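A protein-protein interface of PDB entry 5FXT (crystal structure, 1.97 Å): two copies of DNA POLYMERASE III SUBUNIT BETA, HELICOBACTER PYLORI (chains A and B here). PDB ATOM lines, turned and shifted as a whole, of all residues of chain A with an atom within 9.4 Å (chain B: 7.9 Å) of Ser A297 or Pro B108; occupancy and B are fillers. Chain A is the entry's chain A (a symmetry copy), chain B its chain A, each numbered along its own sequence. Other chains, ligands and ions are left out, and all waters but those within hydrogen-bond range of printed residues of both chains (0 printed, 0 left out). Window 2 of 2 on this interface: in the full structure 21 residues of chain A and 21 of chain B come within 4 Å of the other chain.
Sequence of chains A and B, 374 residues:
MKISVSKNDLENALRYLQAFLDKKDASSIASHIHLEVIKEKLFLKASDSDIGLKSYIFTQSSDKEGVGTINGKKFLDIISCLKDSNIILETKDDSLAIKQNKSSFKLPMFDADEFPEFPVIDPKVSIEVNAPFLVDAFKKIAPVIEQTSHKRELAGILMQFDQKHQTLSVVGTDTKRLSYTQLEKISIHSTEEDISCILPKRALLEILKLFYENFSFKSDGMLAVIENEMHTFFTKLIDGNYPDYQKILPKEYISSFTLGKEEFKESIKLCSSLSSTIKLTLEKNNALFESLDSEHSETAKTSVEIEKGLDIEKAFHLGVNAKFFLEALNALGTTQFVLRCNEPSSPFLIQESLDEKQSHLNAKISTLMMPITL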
ATOM      1  N   LEU A 274      -9.824  12.371   4.650  1.00  0.00           N
ATOM      2  CA  LEU A 274      -8.848  12.989   3.776  1.00  0.00           C
ATOM      3  C   LEU A 274      -8.702  14.475   3.890  1.00  0.00           C
ATOM      4  O   LEU A 274      -7.921  15.034   3.130  1.00  0.00           O
ATOM      5  CB  LEU A 274      -9.213  12.721   2.303  1.00  0.00           C
ATOM      6  CG  LEU A 274      -9.200  11.240   1.958  1.00  0.00           C
ATOM      7  CD1 LEU A 274      -9.684  11.038   0.554  1.00  0.00           C
ATOM      8  CD2 LEU A 274      -7.808  10.650   2.176  1.00  0.00           C
ATOM      9  N   SER A 291     -14.767  16.490   0.593  1.00  0.00           N
ATOM     10  CA  SER A 291     -13.519  16.993   1.125  1.00  0.00           C
ATOM     11  C   SER A 291     -13.084  18.264   0.355  1.00  0.00           C
ATOM     12  O   SER A 291     -13.270  18.383  -0.871  1.00  0.00           O
ATOM     13  CB  SER A 291     -12.437  15.948   1.068  1.00  0.00           C
ATOM     14  OG  SER A 291     -12.412  15.311  -0.213  1.00  0.00           O
ATOM     15  N   ASP A 293     -10.097  20.630   1.767  1.00  0.00           N
ATOM     16  CA  ASP A 293      -8.665  20.926   1.878  1.00  0.00           C
ATOM     17  C   ASP A 293      -7.806  19.699   1.545  1.00  0.00           C
ATOM     18  O   ASP A 293      -6.645  19.680   1.921  1.00  0.00           O
ATOM     19  CB  ASP A 293      -8.300  21.567   3.260  1.00  0.00           C
ATOM     20  CG  ASP A 293      -8.322  20.550   4.438  1.00  0.00           C
ATOM     21  OD1 ASP A 293      -9.213  19.652   4.436  1.00  0.00           O
ATOM     22  OD2 ASP A 293      -7.433  20.617   5.341  1.00  0.00           O
ATOM     23  N   SER A 294      -8.339  18.699   0.820  1.00  0.00           N
ATOM     24  CA  SER A 294      -7.562  17.486   0.533  1.00  0.00           C
ATOM     25  C   SER A 294      -6.406  17.787  -0.428  1.00  0.00           C
ATOM     26  O   SER A 294      -6.427  18.806  -1.125  1.00  0.00           O
ATOM     27  CB  SER A 294      -8.436  16.310   0.022  1.00  0.00           C
ATOM     28  OG  SER A 294      -9.613  16.715  -0.687  1.00  0.00           O
ATOM     29  N   GLU A 295      -5.393  16.907  -0.417  1.00  0.00           N
ATOM     30  CA  GLU A 295      -4.234  16.973  -1.352  1.00  0.00           C
ATOM     31  C   GLU A 295      -4.781  16.707  -2.758  1.00  0.00           C
ATOM     32  O   GLU A 295      -5.675  15.883  -2.902  1.00  0.00           O
ATOM     33  CB  GLU A 295      -3.164  15.924  -0.995  1.00  0.00           C
ATOM     34  CG  GLU A 295      -2.592  15.984   0.431  1.00  0.00           C
ATOM     35  CD  GLU A 295      -1.709  17.192   0.677  1.00  0.00           C
ATOM     36  OE1 GLU A 295      -1.396  17.935  -0.287  1.00  0.00           O
ATOM     37  OE2 GLU A 295      -1.324  17.401   1.846  1.00  0.00           O
ATOM     38  N   HIS A 296      -4.274  17.393  -3.781  1.00  0.00           N
ATOM     39  CA  HIS A 296      -5.133  17.676  -4.958  1.00  0.00           C
ATOM     40  C   HIS A 296      -5.565  16.459  -5.817  1.00  0.00           C
ATOM     41  O   HIS A 296      -6.549  16.574  -6.574  1.00  0.00           O
ATOM     42  CB  HIS A 296      -4.587  18.831  -5.836  1.00  0.00           C
ATOM     43  CG  HIS A 296      -5.668  19.648  -6.499  1.00  0.00           C
ATOM     44  ND1 HIS A 296      -6.011  19.504  -7.831  1.00  0.00           N
ATOM     45  CD2 HIS A 296      -6.495  20.604  -6.005  1.00  0.00           C
ATOM     46  CE1 HIS A 296      -6.991  20.339  -8.130  1.00  0.00           C
ATOM     47  NE2 HIS A 296      -7.304  21.018  -7.040  1.00  0.00           N
ATOM     48  N   SER A 297      -4.876  15.314  -5.683  1.00  0.00           N
ATOM     49  CA  SER A 297      -5.368  14.045  -6.258  1.00  0.00           C
ATOM     50  C   SER A 297      -6.041  13.108  -5.204  1.00  0.00           C
ATOM     51  O   SER A 297      -6.055  11.862  -5.360  1.00  0.00           O
ATOM     52  CB  SER A 297      -4.229  13.342  -7.008  1.00  0.00           C
ATOM     53  OG  SER A 297      -3.827  14.121  -8.144  1.00  0.00           O
ATOM     54  N   GLU A 298      -6.595  13.683  -4.127  1.00  0.00           N
ATOM     55  CA  GLU A 298      -7.306  12.896  -3.136  1.00  0.00           C
ATOM     56  C   GLU A 298      -8.630  13.558  -2.889  1.00  0.00           C
ATOM     57  O   GLU A 298      -8.670  14.755  -2.655  1.00  0.00           O
ATOM     58  CB  GLU A 298      -6.524  12.797  -1.833  1.00  0.00           C
ATOM     59  CG  GLU A 298      -5.077  12.461  -2.042  1.00  0.00           C
ATOM     60  CD  GLU A 298      -4.347  12.295  -0.770  1.00  0.00           C
ATOM     61  OE1 GLU A 298      -4.907  12.689   0.285  1.00  0.00           O
ATOM     62  OE2 GLU A 298      -3.207  11.770  -0.832  1.00  0.00           O
ATOM     63  N   THR A 299      -9.696  12.761  -2.917  1.00  0.00           N
ATOM     64  CA  THR A 299     -11.080  13.227  -2.954  1.00  0.00           C
ATOM     65  C   THR A 299     -11.999  12.308  -2.167  1.00  0.00           C
ATOM     66  O   THR A 299     -11.969  11.117  -2.392  1.00  0.00           O
ATOM     67  CB  THR A 299     -11.482  13.251  -4.409  1.00  0.00           C
ATOM     68  OG1 THR A 299     -11.286  14.558  -4.868  1.00  0.00           O
ATOM     69  CG2 THR A 299     -12.919  12.784  -4.702  1.00  0.00           C
ATOM     70  N   ALA A 300     -12.824  12.853  -1.263  1.00  0.00           N
ATOM     71  CA  ALA A 300     -13.881  12.094  -0.592  1.00  0.00           C
ATOM     72  C   ALA A 300     -15.240  12.785  -0.788  1.00  0.00           C
ATOM     73  O   ALA A 300     -15.341  13.945  -0.508  1.00  0.00           O
ATOM     74  CB  ALA A 300     -13.561  11.941   0.871  1.00  0.00           C
ATOM     75  N   ALA B  26       3.889  10.473   2.841  1.00  0.00           N
ATOM     76  CA  ALA B  26       2.866   9.962   1.904  1.00  0.00           C
ATOM     77  C   ALA B  26       3.288  10.073   0.462  1.00  0.00           C
ATOM     78  O   ALA B  26       2.769   9.353  -0.333  1.00  0.00           O
ATOM     79  CB  ALA B  26       1.491  10.615   2.157  1.00  0.00           C
ATOM     80  N   HIS B  32       2.855   3.068   0.381  1.00  0.00           N
ATOM     81  CA  HIS B  32       1.807   2.433  -0.378  1.00  0.00           C
ATOM     82  C   HIS B  32       1.764   0.882  -0.258  1.00  0.00           C
ATOM     83  O   HIS B  32       2.761   0.272  -0.061  1.00  0.00           O
ATOM     84  CB  HIS B  32       1.944   2.760  -1.894  1.00  0.00           C
ATOM     85  CG  HIS B  32       1.435   4.125  -2.275  1.00  0.00           C
ATOM     86  ND1 HIS B  32       0.745   4.360  -3.440  1.00  0.00           N
ATOM     87  CD2 HIS B  32       1.502   5.312  -1.630  1.00  0.00           C
ATOM     88  CE1 HIS B  32       0.389   5.634  -3.483  1.00  0.00           C
ATOM     89  NE2 HIS B  32       0.867   6.242  -2.415  1.00  0.00           N
ATOM     90  N   GLY B  68      -1.627  -2.116  -9.455  1.00  0.00           N
ATOM     91  CA  GLY B  68      -1.663  -0.684  -9.030  1.00  0.00           C
ATOM     92  C   GLY B  68      -1.092  -0.545  -7.610  1.00  0.00           C
ATOM     93  O   GLY B  68      -0.520  -1.475  -7.068  1.00  0.00           O
ATOM     94  N   THR B  69      -1.206   0.620  -7.022  1.00  0.00           N
ATOM     95  CA  THR B  69      -0.699   0.870  -5.656  1.00  0.00           C
ATOM     96  C   THR B  69      -1.621   1.871  -5.017  1.00  0.00           C
ATOM     97  O   THR B  69      -2.376   2.587  -5.719  1.00  0.00           O
ATOM     98  CB  THR B  69       0.719   1.461  -5.591  1.00  0.00           C
ATOM     99  OG1 THR B  69       0.641   2.897  -5.766  1.00  0.00           O
ATOM    100  CG2 THR B  69       1.643   0.831  -6.613  1.00  0.00           C
ATOM    101  N   ILE B  70      -1.532   1.958  -3.690  1.00  0.00           N
ATOM    102  CA  ILE B  70      -2.340   2.933  -2.962  1.00  0.00           C
ATOM    103  C   ILE B  70      -1.763   3.231  -1.594  1.00  0.00           C
ATOM    104  O   ILE B  70      -1.179   2.348  -0.946  1.00  0.00           O
ATOM    105  CB  ILE B  70      -3.818   2.455  -2.860  1.00  0.00           C
ATOM    106  CG1 ILE B  70      -4.702   3.652  -2.503  1.00  0.00           C
ATOM    107  CG2 ILE B  70      -3.969   1.220  -1.966  1.00  0.00           C
ATOM    108  CD1 ILE B  70      -6.127   3.277  -2.226  1.00  0.00           C
ATOM    109  N   ASN B  71      -1.885   4.468  -1.152  1.00  0.00           N
ATOM    110  CA  ASN B  71      -1.450   4.833   0.170  1.00  0.00           C
ATOM    111  C   ASN B  71      -2.165   4.023   1.262  1.00  0.00           C
ATOM    112  O   ASN B  71      -3.380   4.104   1.422  1.00  0.00           O
ATOM    113  CB  ASN B  71      -1.714   6.328   0.455  1.00  0.00           C
ATOM    114  CG  ASN B  71      -1.136   6.766   1.821  1.00  0.00           C
ATOM    115  OD1 ASN B  71      -1.753   6.598   2.850  1.00  0.00           O
ATOM    116  ND2 ASN B  71       0.082   7.335   1.796  1.00  0.00           N
ATOM    117  N   LYS B  74      -4.236   5.982   4.258  1.00  0.00           N
ATOM    118  CA  LYS B  74      -5.410   6.649   3.776  1.00  0.00           C
ATOM    119  C   LYS B  74      -6.428   5.654   3.367  1.00  0.00           C
ATOM    120  O   LYS B  74      -7.553   5.785   3.744  1.00  0.00           O
ATOM    121  CB  LYS B  74      -5.082   7.604   2.614  1.00  0.00           C
ATOM    122  CG  LYS B  74      -4.161   8.734   2.983  1.00  0.00           C
ATOM    123  CD  LYS B  74      -3.600   9.426   1.727  1.00  0.00           C
ATOM    124  CE  LYS B  74      -2.535  10.462   2.050  1.00  0.00           C
ATOM    125  NZ  LYS B  74      -3.118  11.594   2.821  1.00  0.00           N
ATOM    126  N   ASP B  93      -7.091   5.565 -14.831  1.00  0.00           N
ATOM    127  CA  ASP B  93      -5.731   6.110 -15.015  1.00  0.00           C
ATOM    128  C   ASP B  93      -4.744   5.750 -13.863  1.00  0.00           C
ATOM    129  O   ASP B  93      -4.694   4.595 -13.380  1.00  0.00           O
ATOM    130  CB  ASP B  93      -5.822   7.633 -15.123  1.00  0.00           C
ATOM    131  N   ASP B  94      -3.985   6.746 -13.405  1.00  0.00           N
ATOM    132  CA  ASP B  94      -3.144   6.588 -12.209  1.00  0.00           C
ATOM    133  C   ASP B  94      -3.887   7.011 -10.936  1.00  0.00           C
ATOM    134  O   ASP B  94      -3.296   7.574 -10.025  1.00  0.00           O
ATOM    135  CB  ASP B  94      -1.789   7.292 -12.338  1.00  0.00           C
ATOM    136  CG  ASP B  94      -1.849   8.565 -13.128  1.00  0.00           C
ATOM    137  OD1 ASP B  94      -2.386   9.572 -12.612  1.00  0.00           O
ATOM    138  OD2 ASP B  94      -1.347   8.528 -14.289  1.00  0.00           O
ATOM    139  N   SER B  95      -5.172   6.694 -10.878  1.00  0.00           N
ATOM    140  CA  SER B  95      -5.991   6.922  -9.683  1.00  0.00           C
ATOM    141  C   SER B  95      -6.840   5.687  -9.355  1.00  0.00           C
ATOM    142  O   SER B  95      -7.256   4.938 -10.277  1.00  0.00           O
ATOM    143  CB  SER B  95      -6.840   8.152  -9.914  1.00  0.00           C
ATOM    144  OG  SER B  95      -7.580   8.403  -8.776  1.00  0.00           O
ATOM    145  N   LEU B  96      -7.044   5.423  -8.047  1.00  0.00           N
ATOM    146  CA  LEU B  96      -7.958   4.394  -7.625  1.00  0.00           C
ATOM    147  C   LEU B  96      -9.264   4.978  -7.130  1.00  0.00           C
ATOM    148  O   LEU B  96      -9.267   5.819  -6.213  1.00  0.00           O
ATOM    149  CB  LEU B  96      -7.377   3.550  -6.517  1.00  0.00           C
ATOM    150  CG  LEU B  96      -8.237   2.334  -6.163  1.00  0.00           C
ATOM    151  CD1 LEU B  96      -8.189   1.215  -7.191  1.00  0.00           C
ATOM    152  CD2 LEU B  96      -7.791   1.808  -4.822  1.00  0.00           C
ATOM    153  N   ALA B  97     -10.376   4.471  -7.660  1.00  0.00           N
ATOM    154  CA  ALA B  97     -11.685   4.937  -7.235  1.00  0.00           C
ATOM    155  C   ALA B  97     -12.285   3.925  -6.331  1.00  0.00           C
ATOM    156  O   ALA B  97     -12.143   2.697  -6.563  1.00  0.00           O
ATOM    157  CB  ALA B  97     -12.577   5.292  -8.448  1.00  0.00           C
ATOM    158  N   PHE B 105     -14.628   7.910  -3.423  1.00  0.00           N
ATOM    159  CA  PHE B 105     -13.274   8.437  -3.168  1.00  0.00           C
ATOM    160  C   PHE B 105     -12.329   8.181  -4.338  1.00  0.00           C
ATOM    161  O   PHE B 105     -12.503   7.197  -5.088  1.00  0.00           O
ATOM    162  CB  PHE B 105     -12.674   7.814  -1.941  1.00  0.00           C
ATOM    163  CG  PHE B 105     -13.626   7.665  -0.794  1.00  0.00           C
ATOM    164  CD1 PHE B 105     -14.513   6.590  -0.751  1.00  0.00           C
ATOM    165  CD2 PHE B 105     -13.650   8.605   0.234  1.00  0.00           C
ATOM    166  CE1 PHE B 105     -15.421   6.475   0.262  1.00  0.00           C
ATOM    167  CE2 PHE B 105     -14.540   8.475   1.297  1.00  0.00           C
ATOM    168  CZ  PHE B 105     -15.432   7.401   1.315  1.00  0.00           C
ATOM    169  N   LYS B 106     -11.340   9.065  -4.477  1.00  0.00           N
ATOM    170  CA  LYS B 106     -10.217   8.919  -5.433  1.00  0.00           C
ATOM    171  C   LYS B 106      -8.900   9.107  -4.639  1.00  0.00           C
ATOM    172  O   LYS B 106      -8.773  10.062  -3.834  1.00  0.00           O
ATOM    173  CB  LYS B 106     -10.302   9.903  -6.562  1.00  0.00           C
ATOM    174  N   LEU B 107      -7.967   8.160  -4.803  1.00  0.00           N
ATOM    175  CA  LEU B 107      -6.603   8.303  -4.298  1.00  0.00           C
ATOM    176  C   LEU B 107      -5.571   8.032  -5.423  1.00  0.00           C
ATOM    177  O   LEU B 107      -5.861   7.224  -6.318  1.00  0.00           O
ATOM    178  CB  LEU B 107      -6.392   7.327  -3.141  1.00  0.00           C
ATOM    179  CG  LEU B 107      -6.990   7.605  -1.736  1.00  0.00           C
ATOM    180  CD1 LEU B 107      -6.646   6.487  -0.812  1.00  0.00           C
ATOM    181  CD2 LEU B 107      -6.455   8.866  -1.139  1.00  0.00           C
ATOM    182  N   PRO B 108      -4.372   8.655  -5.356  1.00  0.00           N
ATOM    183  CA  PRO B 108      -3.402   8.488  -6.418  1.00  0.00           C
ATOM    184  C   PRO B 108      -2.613   7.199  -6.256  1.00  0.00           C
ATOM    185  O   PRO B 108      -2.319   6.757  -5.115  1.00  0.00           O
ATOM    186  CB  PRO B 108      -2.551   9.759  -6.315  1.00  0.00           C
ATOM    187  CG  PRO B 108      -2.589  10.115  -4.787  1.00  0.00           C
ATOM    188  CD  PRO B 108      -3.857   9.509  -4.268  1.00  0.00           C
ATOM    189  N   MET B 109      -2.398   6.527  -7.381  1.00  0.00           N
ATOM    190  CA  MET B 109      -1.554   5.302  -7.458  1.00  0.00           C
ATOM    191  C   MET B 109      -0.138   5.745  -7.897  1.00  0.00           C
ATOM    192  O   MET B 109       0.040   6.807  -8.514  1.00  0.00           O
ATOM    193  CB  MET B 109      -2.106   4.287  -8.435  1.00  0.00           C
ATOM    194  CG  MET B 109      -3.576   3.954  -8.287  1.00  0.00           C
ATOM    195  SD  MET B 109      -3.979   2.302  -8.749  1.00  0.00           S
ATOM    196  CE  MET B 109      -3.517   2.181 -10.476  1.00  0.00           C
ATOM    197  N   PHE B 110       0.867   4.974  -7.528  1.00  0.00           N
ATOM    198  CA  PHE B 110       2.218   5.238  -7.949  1.00  0.00           C
ATOM    199  C   PHE B 110       2.555   4.153  -8.963  1.00  0.00           C
ATOM    200  O   PHE B 110       1.769   3.270  -9.246  1.00  0.00           O
ATOM    201  CB  PHE B 110       3.202   5.293  -6.755  1.00  0.00           C
ATOM    202  CG  PHE B 110       3.074   6.504  -5.846  1.00  0.00           C
ATOM    203  CD1 PHE B 110       2.654   7.748  -6.302  1.00  0.00           C
ATOM    204  CD2 PHE B 110       3.454   6.413  -4.503  1.00  0.00           C
ATOM    205  CE1 PHE B 110       2.551   8.837  -5.425  1.00  0.00           C
ATOM    206  CE2 PHE B 110       3.374   7.507  -3.636  1.00  0.00           C
ATOM    207  CZ  PHE B 110       2.917   8.700  -4.087  1.00  0.00           C
ATOM    208  N   ASP B 111       3.698   4.238  -9.575  1.00  0.00           N
ATOM    209  CA  ASP B 111       4.110   3.201 -10.501  1.00  0.00           C
ATOM    210  C   ASP B 111       4.335   1.859  -9.765  1.00  0.00           C
ATOM    211  O   ASP B 111       5.194   1.737  -8.888  1.00  0.00           O
ATOM    212  CB  ASP B 111       5.349   3.730 -11.208  1.00  0.00           C
ATOM    213  CG  ASP B 111       5.911   2.789 -12.232  1.00  0.00           C
ATOM    214  OD1 ASP B 111       5.370   1.695 -12.479  1.00  0.00           O
ATOM    215  OD2 ASP B 111       6.958   3.188 -12.764  1.00  0.00           O
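The backbone carbonyl oxygen (O) of Thr A299 lies within hydrogen-bond range of the backbone NH (N) of Lys B106 (3.0 Å).
The side-chain amino group (NZ) of Lys B74 lies within salt-bridge range of the side-chain carboxylate (OE1) of Glu A298 (3.3 Å).
The backbone NH (N) of Ala A300 sits at hydrogen-bond distance from the side-chain hydroxyl (OG) of Ser A291 (2.7 Å).
The side-chain hydroxyl (OG) of Ser B95 sits at hydrogen-bond distance from the backbone carbonyl oxygen (O) of Leu B107, 3.2 Å away.
The backbone carbonyl oxygen (O) of Glu A298 is in hydrogen-bond range of the side-chain hydroxyl (OG) of Ser A294 (2.9 Å).
N of Lys B74 lies within hydrogen-bond range of OD1 of Asn B71, 2.9 Å away.
The backbone NH of Leu B96 sits at hydrogen-bond distance from the backbone carbonyl oxygen of Leu B107 (2.8 Å).
Among the printed residues, pairs that only touch across the chains: Ser A297 with Lys B106, Ser A297 with Leu B107, Ser A297 with Pro B108, Glu A298 with Lys B106, Glu A298 with Leu B107, Glu A298 with Pro B108, Thr A299 with Phe B105 and Ala A300 with Phe B105.
Gly B68 touches none of the printed residues of chain A.
Of the printed residues of chain A, Lys B74 touches Glu A298.
Printed residues of chain A within 4 Å of Lys B106: Ser A297, Glu A298 and Thr A299.
Pro B108 touches two residues of chain A.
The nearest residue of chain B that does not touch Ser A297 is Ser B95 (5.1 Å).
The nearest residue of chain A that does not touch Pro B108 is Glu A295 (6.8 Å).
The nearest printed residue of chain A that does not touch Lys B106 is Leu A274 (4.6 Å).
Printed residues of chain B that touch a printed residue of chain A: Lys B74, Phe B105, Lys B106, Leu B107 and Pro B108.
Hydrophobic or aromatic side chains of chain B within 4 Å of the printed part of chain A: Phe B105, Leu B107 and Pro B108.
No position is printed for both chains.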
